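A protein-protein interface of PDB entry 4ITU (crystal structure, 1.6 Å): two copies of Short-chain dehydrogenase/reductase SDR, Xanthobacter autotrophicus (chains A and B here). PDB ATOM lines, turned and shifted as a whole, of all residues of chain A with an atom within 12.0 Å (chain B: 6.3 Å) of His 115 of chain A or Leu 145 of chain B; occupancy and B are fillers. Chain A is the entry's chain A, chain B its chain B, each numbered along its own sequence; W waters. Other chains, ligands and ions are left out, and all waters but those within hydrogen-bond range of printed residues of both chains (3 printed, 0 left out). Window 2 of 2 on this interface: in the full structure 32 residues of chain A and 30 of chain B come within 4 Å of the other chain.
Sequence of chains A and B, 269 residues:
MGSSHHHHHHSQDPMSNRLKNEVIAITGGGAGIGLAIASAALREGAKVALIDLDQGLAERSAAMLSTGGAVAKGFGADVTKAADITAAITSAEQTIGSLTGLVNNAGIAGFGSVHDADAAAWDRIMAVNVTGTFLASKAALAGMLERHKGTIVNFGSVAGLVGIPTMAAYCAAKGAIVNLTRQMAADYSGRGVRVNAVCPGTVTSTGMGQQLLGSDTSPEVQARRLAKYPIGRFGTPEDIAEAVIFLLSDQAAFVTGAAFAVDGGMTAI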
ATOM      1  N   PHE A 111      15.588  13.292   6.277  1.00  0.00           N
ATOM      2  CA  PHE A 111      14.268  12.902   5.819  1.00  0.00           C
ATOM      3  C   PHE A 111      13.211  13.822   6.365  1.00  0.00           C
ATOM      4  O   PHE A 111      13.393  14.444   7.418  1.00  0.00           O
ATOM      5  CB  PHE A 111      13.978  11.468   6.233  1.00  0.00           C
ATOM      6  CG  PHE A 111      14.894  10.489   5.593  1.00  0.00           C
ATOM      7  CD1 PHE A 111      14.598   9.972   4.343  1.00  0.00           C
ATOM      8  CD2 PHE A 111      16.084  10.126   6.209  1.00  0.00           C
ATOM      9  CE1 PHE A 111      15.454   9.084   3.725  1.00  0.00           C
ATOM     10  CE2 PHE A 111      16.947   9.248   5.596  1.00  0.00           C
ATOM     11  CZ  PHE A 111      16.632   8.725   4.350  1.00  0.00           C
ATOM     12  N   GLY A 112      12.101  13.898   5.643  1.00  0.00           N
ATOM     13  CA  GLY A 112      10.977  14.712   6.045  1.00  0.00           C
ATOM     14  C   GLY A 112      10.245  15.233   4.823  1.00  0.00           C
ATOM     15  O   GLY A 112      10.857  15.772   3.898  1.00  0.00           O
ATOM     16  N   SER A 113       8.929  15.075   4.820  1.00  0.00           N
ATOM     17  CA  SER A 113       8.103  15.612   3.758  1.00  0.00           C
ATOM     18  C   SER A 113       7.694  17.022   4.141  1.00  0.00           C
ATOM     19  O   SER A 113       7.847  17.422   5.300  1.00  0.00           O
ATOM     20  CB  SER A 113       6.877  14.730   3.563  1.00  0.00           C
ATOM     21  OG  SER A 113       7.265  13.414   3.218  1.00  0.00           O
ATOM     22  N   VAL A 114       7.180  17.786   3.183  1.00  0.00           N
ATOM     23  CA  VAL A 114       6.769  19.161   3.468  1.00  0.00           C
ATOM     24  C   VAL A 114       5.792  19.248   4.644  1.00  0.00           C
ATOM     25  O   VAL A 114       5.847  20.197   5.422  1.00  0.00           O
ATOM     26  CB  VAL A 114       6.174  19.811   2.228  1.00  0.00           C
ATOM     27  N   HIS A 115       4.907  18.263   4.790  1.00  0.00           N
ATOM     28  CA  HIS A 115       3.855  18.377   5.802  1.00  0.00           C
ATOM     29  C   HIS A 115       4.332  18.124   7.227  1.00  0.00           C
ATOM     30  O   HIS A 115       3.658  18.526   8.182  1.00  0.00           O
ATOM     31  CB  HIS A 115       2.662  17.474   5.476  1.00  0.00           C
ATOM     32  CG  HIS A 115       2.897  16.029   5.768  1.00  0.00           C
ATOM     33  ND1 HIS A 115       3.615  15.193   4.949  1.00  0.00           N
ATOM     34  CD2 HIS A 115       2.469  15.256   6.809  1.00  0.00           C
ATOM     35  CE1 HIS A 115       3.638  13.983   5.453  1.00  0.00           C
ATOM     36  NE2 HIS A 115       2.949  13.984   6.585  1.00  0.00           N
ATOM     37  N   ASP A 116       5.478  17.460   7.380  1.00  0.00           N
ATOM     38  CA  ASP A 116       5.963  17.111   8.714  1.00  0.00           C
ATOM     39  C   ASP A 116       7.439  17.408   8.959  1.00  0.00           C
ATOM     40  O   ASP A 116       7.946  17.124  10.043  1.00  0.00           O
ATOM     41  CB  ASP A 116       5.671  15.635   9.026  1.00  0.00           C
ATOM     42  CG  ASP A 116       6.382  14.671   8.082  1.00  0.00           C
ATOM     43  OD1 ASP A 116       7.183  15.115   7.228  1.00  0.00           O
ATOM     44  OD2 ASP A 116       6.145  13.447   8.198  1.00  0.00           O
ATOM     45  N   ALA A 117       8.136  17.971   7.975  1.00  0.00           N
ATOM     46  CA  ALA A 117       9.577  18.188   8.134  1.00  0.00           C
ATOM     47  C   ALA A 117       9.842  19.232   9.212  1.00  0.00           C
ATOM     48  O   ALA A 117       9.125  20.232   9.304  1.00  0.00           O
ATOM     49  CB  ALA A 117      10.218  18.620   6.820  1.00  0.00           C
ATOM     50  N   ASP A 118      10.866  19.001  10.028  1.00  0.00           N
ATOM     51  CA  ASP A 118      11.254  19.989  11.027  1.00  0.00           C
ATOM     52  C   ASP A 118      11.955  21.163  10.365  1.00  0.00           C
ATOM     53  O   ASP A 118      12.894  20.967   9.592  1.00  0.00           O
ATOM     54  CB  ASP A 118      12.171  19.385  12.076  1.00  0.00           C
ATOM     55  CG  ASP A 118      12.693  20.427  13.043  1.00  0.00           C
ATOM     56  OD1 ASP A 118      11.946  20.819  13.977  1.00  0.00           O
ATOM     57  OD2 ASP A 118      13.848  20.863  12.859  1.00  0.00           O
ATOM     58  N   ALA A 119      11.499  22.374  10.662  1.00  0.00           N
ATOM     59  CA  ALA A 119      12.038  23.571  10.020  1.00  0.00           C
ATOM     60  C   ALA A 119      13.530  23.788  10.292  1.00  0.00           C
ATOM     61  O   ALA A 119      14.253  24.277   9.427  1.00  0.00           O
ATOM     62  CB  ALA A 119      11.229  24.799  10.414  1.00  0.00           C
ATOM     63  N   ALA A 120      13.999  23.440  11.488  1.00  0.00           N
ATOM     64  CA  ALA A 120      15.422  23.617  11.799  1.00  0.00           C
ATOM     65  C   ALA A 120      16.291  22.659  10.983  1.00  0.00           C
ATOM     66  O   ALA A 120      17.356  23.037  10.496  1.00  0.00           O
ATOM     67  CB  ALA A 120      15.683  23.442  13.295  1.00  0.00           C
ATOM     68  N   ALA A 121      15.833  21.417  10.842  1.00  0.00           N
ATOM     69  CA  ALA A 121      16.537  20.429  10.028  1.00  0.00           C
ATOM     70  C   ALA A 121      16.553  20.874   8.568  1.00  0.00           C
ATOM     71  O   ALA A 121      17.571  20.743   7.881  1.00  0.00           O
ATOM     72  CB  ALA A 121      15.888  19.061  10.163  1.00  0.00           C
ATOM     73  N   TRP A 122      15.416  21.389   8.105  1.00  0.00           N
ATOM     74  CA  TRP A 122      15.292  21.917   6.747  1.00  0.00           C
ATOM     75  C   TRP A 122      16.380  22.963   6.513  1.00  0.00           C
ATOM     76  O   TRP A 122      17.128  22.893   5.531  1.00  0.00           O
ATOM     77  CB  TRP A 122      13.911  22.549   6.551  1.00  0.00           C
ATOM     78  CG  TRP A 122      13.692  23.140   5.183  1.00  0.00           C
ATOM     79  CD1 TRP A 122      14.212  24.303   4.696  1.00  0.00           C
ATOM     80  CD2 TRP A 122      12.871  22.585   4.143  1.00  0.00           C
ATOM     81  NE1 TRP A 122      13.766  24.504   3.409  1.00  0.00           N
ATOM     82  CE2 TRP A 122      12.950  23.479   3.047  1.00  0.00           C
ATOM     83  CE3 TRP A 122      12.079  21.443   4.030  1.00  0.00           C
ATOM     84  CZ2 TRP A 122      12.268  23.234   1.844  1.00  0.00           C
ATOM     85  CZ3 TRP A 122      11.400  21.206   2.845  1.00  0.00           C
ATOM     86  CH2 TRP A 122      11.499  22.103   1.765  1.00  0.00           C
ATOM     87  N   ILE A 164      12.270  12.766  -4.834  1.00  0.00           N
ATOM     88  CA  ILE A 164      12.491  11.553  -4.061  1.00  0.00           C
ATOM     89  C   ILE A 164      11.533  11.564  -2.888  1.00  0.00           C
ATOM     90  O   ILE A 164      11.517  12.529  -2.132  1.00  0.00           O
ATOM     91  CB  ILE A 164      13.932  11.494  -3.507  1.00  0.00           C
ATOM     92  CG1 ILE A 164      14.963  11.689  -4.621  1.00  0.00           C
ATOM     93  CG2 ILE A 164      14.172  10.174  -2.756  1.00  0.00           C
ATOM     94  CD1 ILE A 164      14.885  10.650  -5.727  1.00  0.00           C
ATOM     95  N   PRO A 165      10.718  10.503  -2.737  1.00  0.00           N
ATOM     96  CA  PRO A 165       9.770  10.464  -1.617  1.00  0.00           C
ATOM     97  C   PRO A 165      10.441  10.734  -0.276  1.00  0.00           C
ATOM     98  O   PRO A 165      11.545  10.228  -0.020  1.00  0.00           O
ATOM     99  CB  PRO A 165       9.235   9.026  -1.651  1.00  0.00           C
ATOM    100  CG  PRO A 165       9.386   8.592  -3.075  1.00  0.00           C
ATOM    101  CD  PRO A 165      10.591   9.334  -3.629  1.00  0.00           C
ATOM    102  N   THR A 166       9.792  11.560   0.543  1.00  0.00           N
ATOM    103  CA  THR A 166      10.217  11.864   1.917  1.00  0.00           C
ATOM    104  C   THR A 166      11.565  12.571   2.064  1.00  0.00           C
ATOM    105  O   THR A 166      12.164  12.535   3.134  1.00  0.00           O
ATOM    106  CB  THR A 166      10.253  10.605   2.818  1.00  0.00           C
ATOM    107  OG1 THR A 166      11.451   9.870   2.553  1.00  0.00           O
ATOM    108  CG2 THR A 166       9.042   9.717   2.563  1.00  0.00           C
ATOM    109  N   MET A 167      12.046  13.227   1.014  1.00  0.00           N
ATOM    110  CA  MET A 167      13.273  14.012   1.148  1.00  0.00           C
ATOM    111  C   MET A 167      13.093  15.424   0.625  1.00  0.00           C
ATOM    112  O   MET A 167      13.784  15.846  -0.310  1.00  0.00           O
ATOM    113  CB  MET A 167      14.433  13.324   0.438  1.00  0.00           C
ATOM    114  CG  MET A 167      14.735  11.930   0.956  1.00  0.00           C
ATOM    115  SD  MET A 167      16.238  11.259   0.212  1.00  0.00           S
ATOM    116  CE  MET A 167      17.502  12.060   1.199  1.00  0.00           C
ATOM    117  N   ALA A 168      12.168  16.169   1.222  1.00  0.00           N
ATOM    118  CA  ALA A 168      11.819  17.485   0.703  1.00  0.00           C
ATOM    119  C   ALA A 168      12.970  18.497   0.748  1.00  0.00           C
ATOM    120  O   ALA A 168      13.295  19.105  -0.277  1.00  0.00           O
ATOM    121  CB  ALA A 168      10.600  18.028   1.427  1.00  0.00           C
ATOM    122  N   ALA A 169      13.571  18.695   1.923  1.00  0.00           N
ATOM    123  CA  ALA A 169      14.665  19.664   2.050  1.00  0.00           C
ATOM    124  C   ALA A 169      15.838  19.299   1.143  1.00  0.00           C
ATOM    125  O   ALA A 169      16.410  20.172   0.470  1.00  0.00           O
ATOM    126  CB  ALA A 169      15.123  19.783   3.497  1.00  0.00           C
ATOM    127  N   TYR A 170      16.188  18.018   1.112  1.00  0.00           N
ATOM    128  CA  TYR A 170      17.313  17.542   0.312  1.00  0.00           C
ATOM    129  C   TYR A 170      17.054  17.730  -1.195  1.00  0.00           C
ATOM    130  O   TYR A 170      17.948  18.184  -1.921  1.00  0.00           O
ATOM    131  CB  TYR A 170      17.646  16.085   0.660  1.00  0.00           C
ATOM    132  CG  TYR A 170      18.929  15.559   0.029  1.00  0.00           C
ATOM    133  CD1 TYR A 170      20.183  15.939   0.511  1.00  0.00           C
ATOM    134  CD2 TYR A 170      18.882  14.681  -1.041  1.00  0.00           C
ATOM    135  CE1 TYR A 170      21.355  15.456  -0.068  1.00  0.00           C
ATOM    136  CE2 TYR A 170      20.043  14.188  -1.624  1.00  0.00           C
ATOM    137  CZ  TYR A 170      21.272  14.572  -1.132  1.00  0.00           C
ATOM    138  OH  TYR A 170      22.409  14.070  -1.726  1.00  0.00           O
ATOM    139  N   PHE B 134       7.751  26.062   1.447  1.00  0.00           N
ATOM    140  CA  PHE B 134       7.726  24.986   2.434  1.00  0.00           C
ATOM    141  C   PHE B 134       6.704  25.255   3.546  1.00  0.00           C
ATOM    142  O   PHE B 134       5.805  24.442   3.768  1.00  0.00           O
ATOM    143  CB  PHE B 134       9.150  24.781   2.978  1.00  0.00           C
ATOM    144  CG  PHE B 134       9.226  24.032   4.284  1.00  0.00           C
ATOM    145  CD1 PHE B 134       8.540  22.836   4.489  1.00  0.00           C
ATOM    146  CD2 PHE B 134      10.038  24.519   5.305  1.00  0.00           C
ATOM    147  CE1 PHE B 134       8.638  22.150   5.710  1.00  0.00           C
ATOM    148  CE2 PHE B 134      10.139  23.844   6.522  1.00  0.00           C
ATOM    149  CZ  PHE B 134       9.441  22.660   6.719  1.00  0.00           C
ATOM    150  N   SER B 137       2.950  25.561   2.391  1.00  0.00           N
ATOM    151  CA  SER B 137       2.473  24.240   2.004  1.00  0.00           C
ATOM    152  C   SER B 137       2.242  23.374   3.234  1.00  0.00           C
ATOM    153  O   SER B 137       1.244  22.667   3.311  1.00  0.00           O
ATOM    154  CB  SER B 137       3.462  23.544   1.066  1.00  0.00           C
ATOM    155  OG  SER B 137       3.556  24.233  -0.164  1.00  0.00           O
ATOM    156  N   LYS B 138       3.164  23.430   4.192  1.00  0.00           N
ATOM    157  CA  LYS B 138       3.047  22.652   5.423  1.00  0.00           C
ATOM    158  C   LYS B 138       1.726  22.940   6.128  1.00  0.00           C
ATOM    159  O   LYS B 138       1.023  22.022   6.564  1.00  0.00           O
ATOM    160  CB  LYS B 138       4.238  22.950   6.342  1.00  0.00           C
ATOM    161  CG  LYS B 138       4.197  22.229   7.680  1.00  0.00           C
ATOM    162  CD  LYS B 138       5.565  22.298   8.370  1.00  0.00           C
ATOM    163  CE  LYS B 138       5.521  21.599   9.714  1.00  0.00           C
ATOM    164  NZ  LYS B 138       6.806  21.763  10.444  1.00  0.00           N
ATOM    165  N   ALA B 140      -1.066  24.216   4.805  1.00  0.00           N
ATOM    166  CA  ALA B 140      -2.205  23.833   3.967  1.00  0.00           C
ATOM    167  C   ALA B 140      -2.369  22.323   3.851  1.00  0.00           C
ATOM    168  O   ALA B 140      -3.483  21.816   3.707  1.00  0.00           O
ATOM    169  CB  ALA B 140      -2.060  24.449   2.587  1.00  0.00           C
ATOM    170  N   LEU B 141      -1.260  21.599   3.903  1.00  0.00           N
ATOM    171  CA  LEU B 141      -1.288  20.154   3.659  1.00  0.00           C
ATOM    172  C   LEU B 141      -2.017  19.368   4.737  1.00  0.00           C
ATOM    173  O   LEU B 141      -2.590  18.320   4.454  1.00  0.00           O
ATOM    174  CB  LEU B 141       0.131  19.608   3.483  1.00  0.00           C
ATOM    175  CG  LEU B 141       0.675  19.826   2.071  1.00  0.00           C
ATOM    176  CD1 LEU B 141       2.179  19.654   2.059  1.00  0.00           C
ATOM    177  CD2 LEU B 141       0.030  18.833   1.118  1.00  0.00           C
ATOM    178  N   ALA B 142      -1.992  19.857   5.972  1.00  0.00           N
ATOM    179  CA  ALA B 142      -2.717  19.173   7.044  1.00  0.00           C
ATOM    180  C   ALA B 142      -4.163  18.909   6.633  1.00  0.00           C
ATOM    181  O   ALA B 142      -4.611  17.755   6.599  1.00  0.00           O
ATOM    182  CB  ALA B 142      -2.662  19.989   8.320  1.00  0.00           C
ATOM    183  N   GLY B 143      -4.874  19.968   6.266  1.00  0.00           N
ATOM    184  CA  GLY B 143      -6.262  19.844   5.844  1.00  0.00           C
ATOM    185  C   GLY B 143      -6.429  19.132   4.513  1.00  0.00           C
ATOM    186  O   GLY B 143      -7.314  18.295   4.353  1.00  0.00           O
ATOM    187  N   MET B 144      -5.587  19.466   3.538  1.00  0.00           N
ATOM    188  CA  MET B 144      -5.719  18.857   2.217  1.00  0.00           C
ATOM    189  C   MET B 144      -5.547  17.345   2.270  1.00  0.00           C
ATOM    190  O   MET B 144      -6.300  16.612   1.627  1.00  0.00           O
ATOM    191  CB  MET B 144      -4.713  19.468   1.237  1.00  0.00           C
ATOM    192  CG  MET B 144      -5.017  20.911   0.865  1.00  0.00           C
ATOM    193  SD  MET B 144      -3.784  21.539  -0.289  1.00  0.00           S
ATOM    194  CE  MET B 144      -4.527  23.098  -0.734  1.00  0.00           C
ATOM    195  N   LEU B 145      -4.571  16.879   3.037  1.00  0.00           N
ATOM    196  CA  LEU B 145      -4.318  15.448   3.140  1.00  0.00           C
ATOM    197  C   LEU B 145      -5.431  14.766   3.921  1.00  0.00           C
ATOM    198  O   LEU B 145      -5.810  13.641   3.618  1.00  0.00           O
ATOM    199  CB  LEU B 145      -2.966  15.182   3.799  1.00  0.00           C
ATOM    200  CG  LEU B 145      -1.713  15.577   3.015  1.00  0.00           C
ATOM    201  CD1 LEU B 145      -0.490  15.468   3.921  1.00  0.00           C
ATOM    202  CD2 LEU B 145      -1.556  14.697   1.787  1.00  0.00           C
ATOM    203  N   GLU B 146      -5.954  15.467   4.922  1.00  0.00           N
ATOM    204  CA  GLU B 146      -7.065  14.972   5.721  1.00  0.00           C
ATOM    205  C   GLU B 146      -8.270  14.733   4.814  1.00  0.00           C
ATOM    206  O   GLU B 146      -9.017  13.769   4.983  1.00  0.00           O
ATOM    207  CB  GLU B 146      -7.399  16.006   6.795  1.00  0.00           C
ATOM    208  CG  GLU B 146      -8.214  15.498   7.962  1.00  0.00           C
ATOM    209  CD  GLU B 146      -8.322  16.544   9.064  1.00  0.00           C
ATOM    210  OE1 GLU B 146      -7.472  16.544   9.983  1.00  0.00           O
ATOM    211  OE2 GLU B 146      -9.251  17.377   8.996  1.00  0.00           O
ATOM    212  N   ARG B 147      -8.431  15.607   3.824  1.00  0.00           N
ATOM    213  CA  ARG B 147      -9.576  15.558   2.920  1.00  0.00           C
ATOM    214  C   ARG B 147      -9.287  14.831   1.603  1.00  0.00           C
ATOM    215  O   ARG B 147     -10.169  14.719   0.744  1.00  0.00           O
ATOM    216  CB  ARG B 147     -10.068  16.985   2.636  1.00  0.00           C
ATOM    217  CG  ARG B 147     -10.559  17.741   3.878  1.00  0.00           C
ATOM    218  CD  ARG B 147     -11.097  19.127   3.519  1.00  0.00           C
ATOM    219  NE  ARG B 147     -10.060  20.063   3.077  1.00  0.00           N
ATOM    220  CZ  ARG B 147      -9.298  20.780   3.899  1.00  0.00           C
ATOM    221  NH1 ARG B 147      -9.439  20.660   5.215  1.00  0.00           N
ATOM    222  NH2 ARG B 147      -8.388  21.616   3.412  1.00  0.00           N
ATOM    223  N   HIS B 148      -8.062  14.337   1.451  1.00  0.00           N
ATOM    224  CA  HIS B 148      -7.626  13.678   0.217  1.00  0.00           C
ATOM    225  C   HIS B 148      -7.908  14.524  -1.025  1.00  0.00           C
ATOM    226  O   HIS B 148      -8.318  13.998  -2.071  1.00  0.00           O
ATOM    227  CB  HIS B 148      -8.289  12.307   0.065  1.00  0.00           C
ATOM    228  CG  HIS B 148      -7.899  11.330   1.119  1.00  0.00           C
ATOM    229  ND1 HIS B 148      -6.718  10.604   1.070  1.00  0.00           N
ATOM    230  CD2 HIS B 148      -8.514  10.944   2.264  1.00  0.00           C
ATOM    231  CE1 HIS B 148      -6.636   9.824   2.125  1.00  0.00           C
ATOM    232  NE2 HIS B 148      -7.714  10.014   2.874  1.00  0.00           N
ATOM    233  N   LYS B 149      -7.676  15.829  -0.916  1.00  0.00           N
ATOM    234  CA  LYS B 149      -8.089  16.759  -1.966  1.00  0.00           C
ATOM    235  C   LYS B 149      -7.357  18.092  -1.855  1.00  0.00           C
ATOM    236  O   LYS B 149      -7.498  18.817  -0.870  1.00  0.00           O
ATOM    237  CB  LYS B 149      -9.610  16.975  -1.900  1.00  0.00           C
ATOM    238  CG  LYS B 149     -10.178  18.031  -2.859  1.00  0.00           C
ATOM    239  CD  LYS B 149     -10.496  17.440  -4.217  1.00  0.00           C
ATOM    240  CE  LYS B 149     -11.485  18.305  -5.008  1.00  0.00           C
ATOM    241  NZ  LYS B 149     -12.861  18.195  -4.459  1.00  0.00           N
ATOM    242  N   ASP B 187       5.424  12.739  -3.153  1.00  0.00           N
ATOM    243  CA  ASP B 187       4.841  12.354  -1.868  1.00  0.00           C
ATOM    244  C   ASP B 187       3.314  12.339  -1.893  1.00  0.00           C
ATOM    245  O   ASP B 187       2.691  11.470  -1.279  1.00  0.00           O
ATOM    246  CB  ASP B 187       5.280  13.313  -0.752  1.00  0.00           C
ATOM    247  CG  ASP B 187       6.663  12.991  -0.181  1.00  0.00           C
ATOM    248  OD1 ASP B 187       7.175  11.871  -0.389  1.00  0.00           O
ATOM    249  OD2 ASP B 187       7.231  13.880   0.498  1.00  0.00           O
ATOM    250  N   TYR B 188       2.714  13.303  -2.587  1.00  0.00           N
ATOM    251  CA  TYR B 188       1.305  13.626  -2.342  1.00  0.00           C
ATOM    252  C   TYR B 188       0.319  13.352  -3.469  1.00  0.00           C
ATOM    253  O   TYR B 188      -0.896  13.377  -3.234  1.00  0.00           O
ATOM    254  CB  TYR B 188       1.186  15.086  -1.904  1.00  0.00           C
ATOM    255  CG  TYR B 188       1.991  15.403  -0.666  1.00  0.00           C
ATOM    256  CD1 TYR B 188       1.870  14.630   0.485  1.00  0.00           C
ATOM    257  CD2 TYR B 188       2.888  16.464  -0.654  1.00  0.00           C
ATOM    258  CE1 TYR B 188       2.607  14.921   1.626  1.00  0.00           C
ATOM    259  CE2 TYR B 188       3.631  16.752   0.477  1.00  0.00           C
ATOM    260  CZ  TYR B 188       3.488  15.976   1.605  1.00  0.00           C
ATOM    261  OH  TYR B 188       4.220  16.272   2.728  1.00  0.00           O
ATOM    262  N   ARG B 191      -2.083  10.755  -2.780  1.00  0.00           N
ATOM    263  CA  ARG B 191      -2.888  11.050  -1.599  1.00  0.00           C
ATOM    264  C   ARG B 191      -3.920  12.138  -1.892  1.00  0.00           C
ATOM    265  O   ARG B 191      -4.546  12.680  -0.979  1.00  0.00           O
ATOM    266  CB  ARG B 191      -1.979  11.459  -0.435  1.00  0.00           C
ATOM    267  CG  ARG B 191      -0.971  10.364  -0.056  1.00  0.00           C
ATOM    268  CD  ARG B 191      -0.110  10.759   1.134  1.00  0.00           C
ATOM    269  NE  ARG B 191      -0.910  10.906   2.347  1.00  0.00           N
ATOM    270  CZ  ARG B 191      -0.422  11.317   3.515  1.00  0.00           C
ATOM    271  NH1 ARG B 191       0.865  11.619   3.620  1.00  0.00           N
ATOM    272  NH2 ARG B 191      -1.217  11.433   4.574  1.00  0.00           N
ATOM    273  N   GLY B 192      -4.092  12.456  -3.170  1.00  0.00           N
ATOM    274  CA  GLY B 192      -5.150  13.353  -3.606  1.00  0.00           C
ATOM    275  C   GLY B 192      -4.737  14.808  -3.754  1.00  0.00           C
ATOM    276  O   GLY B 192      -5.587  15.670  -3.952  1.00  0.00           O
ATOM    277  N   VAL B 193      -3.444  15.096  -3.636  1.00  0.00           N
ATOM    278  CA  VAL B 193      -2.963  16.471  -3.731  1.00  0.00           C
ATOM    279  C   VAL B 193      -1.975  16.628  -4.881  1.00  0.00           C
ATOM    280  O   VAL B 193      -0.850  16.118  -4.814  1.00  0.00           O
ATOM    281  CB  VAL B 193      -2.285  16.927  -2.417  1.00  0.00           C
ATOM    282  CG1 VAL B 193      -1.826  18.386  -2.532  1.00  0.00           C
ATOM    283  CG2 VAL B 193      -3.239  16.750  -1.232  1.00  0.00           C
HETATM  284  O   HOH W   1       9.044  22.877  12.367  1.00  0.00           O
HETATM  285  O   HOH W   2       1.278  19.634   8.121  1.00  0.00           O
HETATM  286  O   HOH W   3       7.106  16.750   0.472  1.00  0.00           O
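Water W2 bridges O of His 115 of chain A (2.6 Å) and O of Lys 138 of chain B (2.9 Å). Water W3 bridges OD2 of Asp 187 of chain B and N of Val 114 of chain A. Water W1 bridges the backbone NH (N) of Ala 119 of chain A (3.0 Å) and the side-chain amino group (NZ) of Lys 138 of chain B (3.2 Å).
Among the printed residues, merely in contact across the chains: Ser 113 of chain A with Tyr 188 of chain B (3.2 Å), Pro 165 of chain A with Asp 187 of chain B (3.2 Å), Val 114 of chain A with Lys 138 of chain B (3.3 Å), Val 114 of chain A with Phe 134 of chain B (3.4 Å), Ala 117 of chain A with Phe 134 of chain B (3.6 Å), Trp 122 of chain A with Phe 134 of chain B (3.6 Å), His 115 of chain A with Lys 138 of chain B (3.8 Å), His 115 of chain A with Leu 141 of chain B (3.9 Å), His 115 of chain A with Leu 145 of chain B (3.9 Å) and Ala 119 of chain A with Phe 134 of chain B (3.99 Å).
Of chain B, only Lys 138 (3.8 Å), Leu 141 (3.9 Å), Leu 145 (3.9 Å) and Tyr 188 (2.5 Å) come within 4 Å of His 115 of chain A. Printed residues of chain A within 4 Å of Leu 145 of chain B: His 115 (3.9 Å). No residue of chain A comes within 4 Å of Ser 137 of chain B. No residue of chain A comes within 4 Å of Ala 142 of chain B. No residue of chain A comes within 4 Å of His 148 of chain B. Of the printed residues of chain A, Tyr 188 of chain B touches Ser 113, Val 114 and His 115. No residue of chain A comes within 4 Å of Gly 192 of chain B. Of the printed residues of chain A, Leu 141 of chain B touches His 115. Of the printed residues of chain B, Trp 122 of chain A touches Phe 134. Printed residues of chain B within 4 Å of Pro 165 of chain A: Asp 187 (3.2 Å). Of the printed residues of chain B, Ala 119 of chain A touches Phe 134. Printed residues of chain B within 4 Å of Thr 166 of chain A: Asp 187. Tyr 170 of chain A touches none of the printed residues of chain B.
N of Val 193 of chain B sits at hydrogen-bond distance from O of Tyr 188 of chain B (3.1 Å). The backbone NH (N) of Ser 113 of chain A sits at hydrogen-bond distance from the side-chain carboxylate (OD1) of Asp 116 of chain A (3.0 Å). The backbone carbonyl oxygen (O) of Thr 166 of chain A sits at hydrogen-bond distance from the backbone NH (N) of Gly 112 of chain A, at 2.9 Å.
No position is printed for both chains.
Of the 19 printed residues of chain A, 8 touch a printed residue of chain B. Of the 18 printed residues of chain B, 6 touch a printed residue of chain A. Printed residues of chain B that touch a printed residue of chain A: Phe 134, Lys 138, Leu 141, Leu 145, Asp 187 and Tyr 188. Hydrophobic or aromatic side chains of chain B that line the printed part of chain A: Phe 134, Leu 141, Leu 145 and Tyr 188. Along chain B the printed residues that touch a printed residue of chain A span positions 134 to 188.
OH of Tyr 188 of chain B is in hydrogen-bond range of N of Val 114 of chain A (3.4 Å). OG of Ser 113 of chain A lies within hydrogen-bond range of OD2 of Asp 187 of chain B (2.8 Å). The backbone NH (N) of Thr 166 of chain A lies within hydrogen-bond range of the side-chain carboxylate (OD1) of Asp 187 of chain B. O of Ala 117 of chain A is in hydrogen-bond range of NZ of Lys 138 of chain B (3.0 Å). The side-chain hydroxyl (OH) of Tyr 188 of chain B sits at hydrogen-bond distance from a ring nitrogen (ND1) of His 115 of chain A, at 2.5 Å.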
